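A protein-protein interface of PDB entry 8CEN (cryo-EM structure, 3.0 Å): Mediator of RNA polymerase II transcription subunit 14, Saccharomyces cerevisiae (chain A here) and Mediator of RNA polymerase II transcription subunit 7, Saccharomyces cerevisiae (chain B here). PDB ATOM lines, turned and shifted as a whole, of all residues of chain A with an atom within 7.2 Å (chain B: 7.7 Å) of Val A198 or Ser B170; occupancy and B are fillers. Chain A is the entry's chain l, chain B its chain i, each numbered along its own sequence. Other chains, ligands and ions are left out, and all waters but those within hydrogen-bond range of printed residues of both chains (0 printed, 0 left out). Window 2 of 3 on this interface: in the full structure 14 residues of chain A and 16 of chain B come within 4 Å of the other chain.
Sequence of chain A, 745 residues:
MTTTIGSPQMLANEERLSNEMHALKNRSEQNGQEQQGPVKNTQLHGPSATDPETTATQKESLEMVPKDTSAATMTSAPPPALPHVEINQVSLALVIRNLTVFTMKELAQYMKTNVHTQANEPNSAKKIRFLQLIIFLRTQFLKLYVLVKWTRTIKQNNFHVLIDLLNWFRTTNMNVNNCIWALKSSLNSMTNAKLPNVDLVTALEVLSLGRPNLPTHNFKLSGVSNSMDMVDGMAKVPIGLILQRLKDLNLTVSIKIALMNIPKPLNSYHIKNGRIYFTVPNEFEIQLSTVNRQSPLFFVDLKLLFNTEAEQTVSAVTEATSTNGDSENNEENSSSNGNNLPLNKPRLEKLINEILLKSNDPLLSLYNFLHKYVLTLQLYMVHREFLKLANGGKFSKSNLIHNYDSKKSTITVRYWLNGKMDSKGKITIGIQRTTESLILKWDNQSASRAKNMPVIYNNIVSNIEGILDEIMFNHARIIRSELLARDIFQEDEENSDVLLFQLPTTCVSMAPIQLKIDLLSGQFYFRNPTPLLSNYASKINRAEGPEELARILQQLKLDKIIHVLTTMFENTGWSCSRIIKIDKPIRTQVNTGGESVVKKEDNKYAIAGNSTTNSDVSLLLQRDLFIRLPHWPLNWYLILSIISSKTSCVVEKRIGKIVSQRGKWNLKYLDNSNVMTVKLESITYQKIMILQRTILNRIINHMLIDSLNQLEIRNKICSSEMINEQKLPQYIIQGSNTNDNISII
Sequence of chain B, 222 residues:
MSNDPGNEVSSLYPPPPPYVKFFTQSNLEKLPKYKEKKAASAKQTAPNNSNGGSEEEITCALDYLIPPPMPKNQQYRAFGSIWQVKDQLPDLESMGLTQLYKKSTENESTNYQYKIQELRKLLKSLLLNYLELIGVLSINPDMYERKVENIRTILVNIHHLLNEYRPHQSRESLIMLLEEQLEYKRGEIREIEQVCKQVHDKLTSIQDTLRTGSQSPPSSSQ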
ATOM      1  N   LEU A 195      -2.151  -0.324   6.695  1.00  0.00           N
ATOM      2  CA  LEU A 195      -1.827   0.519   7.834  1.00  0.00           C
ATOM      3  C   LEU A 195      -1.008   1.684   7.301  1.00  0.00           C
ATOM      4  O   LEU A 195       0.158   1.503   6.930  1.00  0.00           O
ATOM      5  CB  LEU A 195      -1.071  -0.261   8.906  1.00  0.00           C
ATOM      6  CG  LEU A 195      -1.233   0.220  10.348  1.00  0.00           C
ATOM      7  CD1 LEU A 195      -2.703   0.340  10.705  1.00  0.00           C
ATOM      8  CD2 LEU A 195      -0.532  -0.729  11.302  1.00  0.00           C
ATOM      9  N   PRO A 196      -1.588   2.885   7.229  1.00  0.00           N
ATOM     10  CA  PRO A 196      -0.942   3.982   6.495  1.00  0.00           C
ATOM     11  C   PRO A 196       0.300   4.532   7.174  1.00  0.00           C
ATOM     12  O   PRO A 196       0.682   4.090   8.261  1.00  0.00           O
ATOM     13  CB  PRO A 196      -2.044   5.048   6.421  1.00  0.00           C
ATOM     14  CG  PRO A 196      -3.320   4.312   6.697  1.00  0.00           C
ATOM     15  CD  PRO A 196      -2.942   3.249   7.672  1.00  0.00           C
ATOM     16  N   ASN A 197       0.940   5.494   6.516  1.00  0.00           N
ATOM     17  CA  ASN A 197       2.110   6.148   7.080  1.00  0.00           C
ATOM     18  C   ASN A 197       1.730   6.936   8.327  1.00  0.00           C
ATOM     19  O   ASN A 197       0.656   7.541   8.398  1.00  0.00           O
ATOM     20  CB  ASN A 197       2.749   7.073   6.047  1.00  0.00           C
ATOM     21  CG  ASN A 197       4.042   7.689   6.539  1.00  0.00           C
ATOM     22  OD1 ASN A 197       4.751   7.101   7.354  1.00  0.00           O
ATOM     23  ND2 ASN A 197       4.353   8.881   6.048  1.00  0.00           N
ATOM     24  N   VAL A 198       2.621   6.914   9.315  1.00  0.00           N
ATOM     25  CA  VAL A 198       2.343   7.522  10.606  1.00  0.00           C
ATOM     26  C   VAL A 198       2.356   9.045  10.462  1.00  0.00           C
ATOM     27  O   VAL A 198       2.994   9.600   9.555  1.00  0.00           O
ATOM     28  CB  VAL A 198       3.384   7.016  11.624  1.00  0.00           C
ATOM     29  CG1 VAL A 198       4.752   7.679  11.424  1.00  0.00           C
ATOM     30  CG2 VAL A 198       2.881   7.099  13.033  1.00  0.00           C
ATOM     31  N   ASP A 199       1.615   9.735  11.329  1.00  0.00           N
ATOM     32  CA  ASP A 199       1.479  11.190  11.216  1.00  0.00           C
ATOM     33  C   ASP A 199       2.151  11.864  12.412  1.00  0.00           C
ATOM     34  O   ASP A 199       1.502  12.339  13.354  1.00  0.00           O
ATOM     35  CB  ASP A 199       0.025  11.593  11.090  1.00  0.00           C
ATOM     36  CG  ASP A 199      -0.151  12.853  10.272  1.00  0.00           C
ATOM     37  OD1 ASP A 199       0.761  13.706  10.290  1.00  0.00           O
ATOM     38  OD2 ASP A 199      -1.187  12.989   9.593  1.00  0.00           O
ATOM     39  N   LEU A 200       3.474  11.990  12.307  1.00  0.00           N
ATOM     40  CA  LEU A 200       4.243  12.678  13.332  1.00  0.00           C
ATOM     41  C   LEU A 200       3.980  14.174  13.312  1.00  0.00           C
ATOM     42  O   LEU A 200       4.038  14.815  14.362  1.00  0.00           O
ATOM     43  CB  LEU A 200       5.733  12.399  13.146  1.00  0.00           C
ATOM     44  CG  LEU A 200       6.138  10.926  13.102  1.00  0.00           C
ATOM     45  CD1 LEU A 200       7.530  10.783  12.522  1.00  0.00           C
ATOM     46  CD2 LEU A 200       6.067  10.310  14.488  1.00  0.00           C
ATOM     47  N   VAL A 201       3.677  14.740  12.140  1.00  0.00           N
ATOM     48  CA  VAL A 201       3.437  16.178  12.035  1.00  0.00           C
ATOM     49  C   VAL A 201       2.202  16.569  12.837  1.00  0.00           C
ATOM     50  O   VAL A 201       2.245  17.470  13.688  1.00  0.00           O
ATOM     51  CB  VAL A 201       3.295  16.585  10.556  1.00  0.00           C
ATOM     52  CG1 VAL A 201       2.810  18.021  10.437  1.00  0.00           C
ATOM     53  CG2 VAL A 201       4.602  16.377   9.808  1.00  0.00           C
ATOM     54  N   ALA A 203       0.730  14.697  15.106  1.00  0.00           N
ATOM     55  CA  ALA A 203       0.956  14.337  16.504  1.00  0.00           C
ATOM     56  C   ALA A 203       1.713  15.429  17.254  1.00  0.00           C
ATOM     57  O   ALA A 203       1.332  15.795  18.372  1.00  0.00           O
ATOM     58  CB  ALA A 203       1.712  13.016  16.592  1.00  0.00           C
ATOM     59  N   TYR B 165       5.286  -4.572  11.012  1.00  0.00           N
ATOM     60  CA  TYR B 165       6.489  -3.771  10.812  1.00  0.00           C
ATOM     61  C   TYR B 165       6.203  -2.271  10.851  1.00  0.00           C
ATOM     62  O   TYR B 165       7.140  -1.479  10.994  1.00  0.00           O
ATOM     63  CB  TYR B 165       7.143  -4.165   9.486  1.00  0.00           C
ATOM     64  CG  TYR B 165       8.518  -3.584   9.258  1.00  0.00           C
ATOM     65  CD1 TYR B 165       9.635  -4.128   9.875  1.00  0.00           C
ATOM     66  CD2 TYR B 165       8.699  -2.503   8.410  1.00  0.00           C
ATOM     67  CE1 TYR B 165      10.893  -3.598   9.662  1.00  0.00           C
ATOM     68  CE2 TYR B 165       9.946  -1.967   8.192  1.00  0.00           C
ATOM     69  CZ  TYR B 165      11.039  -2.517   8.817  1.00  0.00           C
ATOM     70  OH  TYR B 165      12.281  -1.977   8.591  1.00  0.00           O
ATOM     71  N   ARG B 166       4.934  -1.878  10.718  1.00  0.00           N
ATOM     72  CA  ARG B 166       4.569  -0.460  10.707  1.00  0.00           C
ATOM     73  C   ARG B 166       4.979   0.340  11.948  1.00  0.00           C
ATOM     74  O   ARG B 166       5.406   1.493  11.765  1.00  0.00           O
ATOM     75  CB  ARG B 166       3.061  -0.321  10.450  1.00  0.00           C
ATOM     76  CG  ARG B 166       2.684  -0.096   8.998  1.00  0.00           C
ATOM     77  CD  ARG B 166       3.094   1.288   8.528  1.00  0.00           C
ATOM     78  NE  ARG B 166       2.673   1.533   7.154  1.00  0.00           N
ATOM     79  CZ  ARG B 166       3.173   2.483   6.376  1.00  0.00           C
ATOM     80  NH1 ARG B 166       4.120   3.300   6.805  1.00  0.00           N
ATOM     81  NH2 ARG B 166       2.711   2.614   5.136  1.00  0.00           N
ATOM     82  N   PRO B 167       4.839  -0.140  13.197  1.00  0.00           N
ATOM     83  CA  PRO B 167       5.405   0.639  14.316  1.00  0.00           C
ATOM     84  C   PRO B 167       6.913   0.811  14.245  1.00  0.00           C
ATOM     85  O   PRO B 167       7.426   1.869  14.636  1.00  0.00           O
ATOM     86  CB  PRO B 167       4.989  -0.169  15.552  1.00  0.00           C
ATOM     87  CG  PRO B 167       3.767  -0.863  15.136  1.00  0.00           C
ATOM     88  CD  PRO B 167       4.015  -1.250  13.714  1.00  0.00           C
ATOM     89  N   HIS B 168       7.637  -0.195  13.747  1.00  0.00           N
ATOM     90  CA  HIS B 168       9.081  -0.068  13.585  1.00  0.00           C
ATOM     91  C   HIS B 168       9.428   0.994  12.548  1.00  0.00           C
ATOM     92  O   HIS B 168      10.343   1.799  12.758  1.00  0.00           O
ATOM     93  CB  HIS B 168       9.680  -1.420  13.198  1.00  0.00           C
ATOM     94  CG  HIS B 168      11.119  -1.574  13.579  1.00  0.00           C
ATOM     95  ND1 HIS B 168      11.587  -1.301  14.845  1.00  0.00           N
ATOM     96  CD2 HIS B 168      12.194  -1.979  12.860  1.00  0.00           C
ATOM     97  CE1 HIS B 168      12.888  -1.527  14.891  1.00  0.00           C
ATOM     98  NE2 HIS B 168      13.280  -1.940  13.699  1.00  0.00           N
ATOM     99  N   GLN B 169       8.695   1.024  11.432  1.00  0.00           N
ATOM    100  CA  GLN B 169       8.917   2.056  10.424  1.00  0.00           C
ATOM    101  C   GLN B 169       8.506   3.433  10.932  1.00  0.00           C
ATOM    102  O   GLN B 169       9.126   4.434  10.568  1.00  0.00           O
ATOM    103  CB  GLN B 169       8.157   1.711   9.144  1.00  0.00           C
ATOM    104  CG  GLN B 169       8.581   2.510   7.924  1.00  0.00           C
ATOM    105  CD  GLN B 169       7.712   3.729   7.691  1.00  0.00           C
ATOM    106  OE1 GLN B 169       6.542   3.752   8.066  1.00  0.00           O
ATOM    107  NE2 GLN B 169       8.284   4.752   7.067  1.00  0.00           N
ATOM    108  N   SER B 170       7.475   3.500  11.778  1.00  0.00           N
ATOM    109  CA  SER B 170       7.082   4.767  12.388  1.00  0.00           C
ATOM    110  C   SER B 170       8.169   5.295  13.317  1.00  0.00           C
ATOM    111  O   SER B 170       8.464   6.497  13.327  1.00  0.00           O
ATOM    112  CB  SER B 170       5.773   4.583  13.154  1.00  0.00           C
ATOM    113  OG  SER B 170       4.763   4.061  12.310  1.00  0.00           O
ATOM    114  N   ARG B 171       8.779   4.405  14.100  1.00  0.00           N
ATOM    115  CA  ARG B 171       9.852   4.821  14.993  1.00  0.00           C
ATOM    116  C   ARG B 171      11.109   5.188  14.210  1.00  0.00           C
ATOM    117  O   ARG B 171      11.839   6.110  14.601  1.00  0.00           O
ATOM    118  CB  ARG B 171      10.113   3.711  16.007  1.00  0.00           C
ATOM    119  CG  ARG B 171      10.843   4.136  17.258  1.00  0.00           C
ATOM    120  CD  ARG B 171      10.686   3.080  18.349  1.00  0.00           C
ATOM    121  NE  ARG B 171      10.511   1.738  17.804  1.00  0.00           N
ATOM    122  CZ  ARG B 171       9.454   0.968  18.027  1.00  0.00           C
ATOM    123  NH1 ARG B 171       8.457   1.368  18.799  1.00  0.00           N
ATOM    124  NH2 ARG B 171       9.396  -0.233  17.459  1.00  0.00           N
ATOM    125  N   GLU B 172      11.355   4.507  13.086  1.00  0.00           N
ATOM    126  CA  GLU B 172      12.405   4.932  12.163  1.00  0.00           C
ATOM    127  C   GLU B 172      12.115   6.309  11.579  1.00  0.00           C
ATOM    128  O   GLU B 172      13.034   7.102  11.366  1.00  0.00           O
ATOM    129  CB  GLU B 172      12.572   3.907  11.042  1.00  0.00           C
ATOM    130  CG  GLU B 172      13.284   2.633  11.453  1.00  0.00           C
ATOM    131  CD  GLU B 172      14.720   2.885  11.862  1.00  0.00           C
ATOM    132  OE1 GLU B 172      15.469   3.486  11.064  1.00  0.00           O
ATOM    133  OE2 GLU B 172      15.107   2.477  12.975  1.00  0.00           O
ATOM    134  N   SER B 173      10.845   6.601  11.290  1.00  0.00           N
ATOM    135  CA  SER B 173      10.479   7.921  10.780  1.00  0.00           C
ATOM    136  C   SER B 173      10.691   9.000  11.833  1.00  0.00           C
ATOM    137  O   SER B 173      11.102  10.120  11.510  1.00  0.00           O
ATOM    138  CB  SER B 173       9.029   7.914  10.301  1.00  0.00           C
ATOM    139  OG  SER B 173       8.901   7.218   9.074  1.00  0.00           O
ATOM    140  N   LEU B 174      10.415   8.682  13.101  1.00  0.00           N
ATOM    141  CA  LEU B 174      10.703   9.625  14.181  1.00  0.00           C
ATOM    142  C   LEU B 174      12.207   9.854  14.334  1.00  0.00           C
ATOM    143  O   LEU B 174      12.653  10.992  14.549  1.00  0.00           O
ATOM    144  CB  LEU B 174      10.094   9.121  15.489  1.00  0.00           C
ATOM    145  CG  LEU B 174      10.417   9.911  16.757  1.00  0.00           C
ATOM    146  CD1 LEU B 174       9.776  11.285  16.703  1.00  0.00           C
ATOM    147  CD2 LEU B 174       9.948   9.152  17.986  1.00  0.00           C
ATOM    148  N   ILE B 175      12.997   8.782  14.217  1.00  0.00           N
ATOM    149  CA  ILE B 175      14.454   8.901  14.242  1.00  0.00           C
ATOM    150  C   ILE B 175      14.941   9.753  13.074  1.00  0.00           C
ATOM    151  O   ILE B 175      15.840  10.587  13.226  1.00  0.00           O
ATOM    152  CB  ILE B 175      15.096   7.499  14.243  1.00  0.00           C
ATOM    153  CG1 ILE B 175      14.925   6.836  15.609  1.00  0.00           C
ATOM    154  CG2 ILE B 175      16.574   7.554  13.883  1.00  0.00           C
ATOM    155  CD1 ILE B 175      15.355   5.391  15.638  1.00  0.00           C
ATOM    156  N   MET B 176      14.339   9.567  11.896  1.00  0.00           N
ATOM    157  CA  MET B 176      14.683  10.366  10.723  1.00  0.00           C
ATOM    158  C   MET B 176      14.319  11.832  10.920  1.00  0.00           C
ATOM    159  O   MET B 176      15.045  12.721  10.466  1.00  0.00           O
ATOM    160  CB  MET B 176      13.982   9.800   9.489  1.00  0.00           C
ATOM    161  CG  MET B 176      14.359  10.477   8.181  1.00  0.00           C
ATOM    162  SD  MET B 176      13.511   9.764   6.759  1.00  0.00           S
ATOM    163  CE  MET B 176      14.351   8.188   6.618  1.00  0.00           C
ATOM    164  N   LEU B 177      13.192  12.100  11.585  1.00  0.00           N
ATOM    165  CA  LEU B 177      12.812  13.473  11.911  1.00  0.00           C
ATOM    166  C   LEU B 177      13.840  14.130  12.826  1.00  0.00           C
ATOM    167  O   LEU B 177      14.258  15.272  12.592  1.00  0.00           O
ATOM    168  CB  LEU B 177      11.431  13.482  12.564  1.00  0.00           C
ATOM    169  CG  LEU B 177      10.928  14.824  13.094  1.00  0.00           C
ATOM    170  CD1 LEU B 177      10.716  15.808  11.959  1.00  0.00           C
ATOM    171  CD2 LEU B 177       9.651  14.625  13.887  1.00  0.00           C
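NE of Arg B166 is in hydrogen-bond range of O of Pro A196 (3.4 Å).
NE of Arg B166 lies within hydrogen-bond range of O of Leu A195 (2.5 Å).
The backbone carbonyl oxygen (O) of Arg B166 sits at hydrogen-bond distance from the side-chain hydroxyl (OG) of Ser B170 (2.7 Å).
The backbone carbonyl oxygen (O) of Gln B169 is in hydrogen-bond range of the side-chain hydroxyl (OG) of Ser B173 (3.2 Å).
The guanidinium group of Arg B166 lies within hydrogen-bond range of the side-chain amide oxygen of Gln B169 (2.8 Å).
Of the printed residues of chain B, Leu A195 touches Arg B166 (2.5 Å).
Printed residues of chain B within 4 Å of Asn A197: Arg B166 (3.5 Å) and Gln B169 (3.9 Å).
Val A198 touches just one residue of chain B: Ser B170.
Printed residues of chain A within 4 Å of Arg B166: Leu A195, Pro A196 and Asn A197.
Of chain A, only Val A198 comes within 4 Å of Ser B170.
Of the printed residues of chain A, Ser B173 touches Leu A200.
Printed residues of chain A within 4 Å of Leu B174: Leu A200.
The nearest residue of chain A that does not touch Ser B170 is Leu A200 (4.5 Å).
The nearest printed residue of chain A that does not touch Ser B173 is Val A198 (4.4 Å).
Among the printed residues, merely in contact across the chains: Val A198 with Ser B170, Asn A197 with Arg B166, Leu A200 with Leu B174, Leu A200 with Ser B173 and Asn A197 with Gln B169.
Of the 8 printed residues of chain A, 5 touch a printed residue of chain B.
Hydrophobic or aromatic side chains of chain A within 4 Å of the printed part of chain B: Leu A195, Val A198 and Leu A200.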
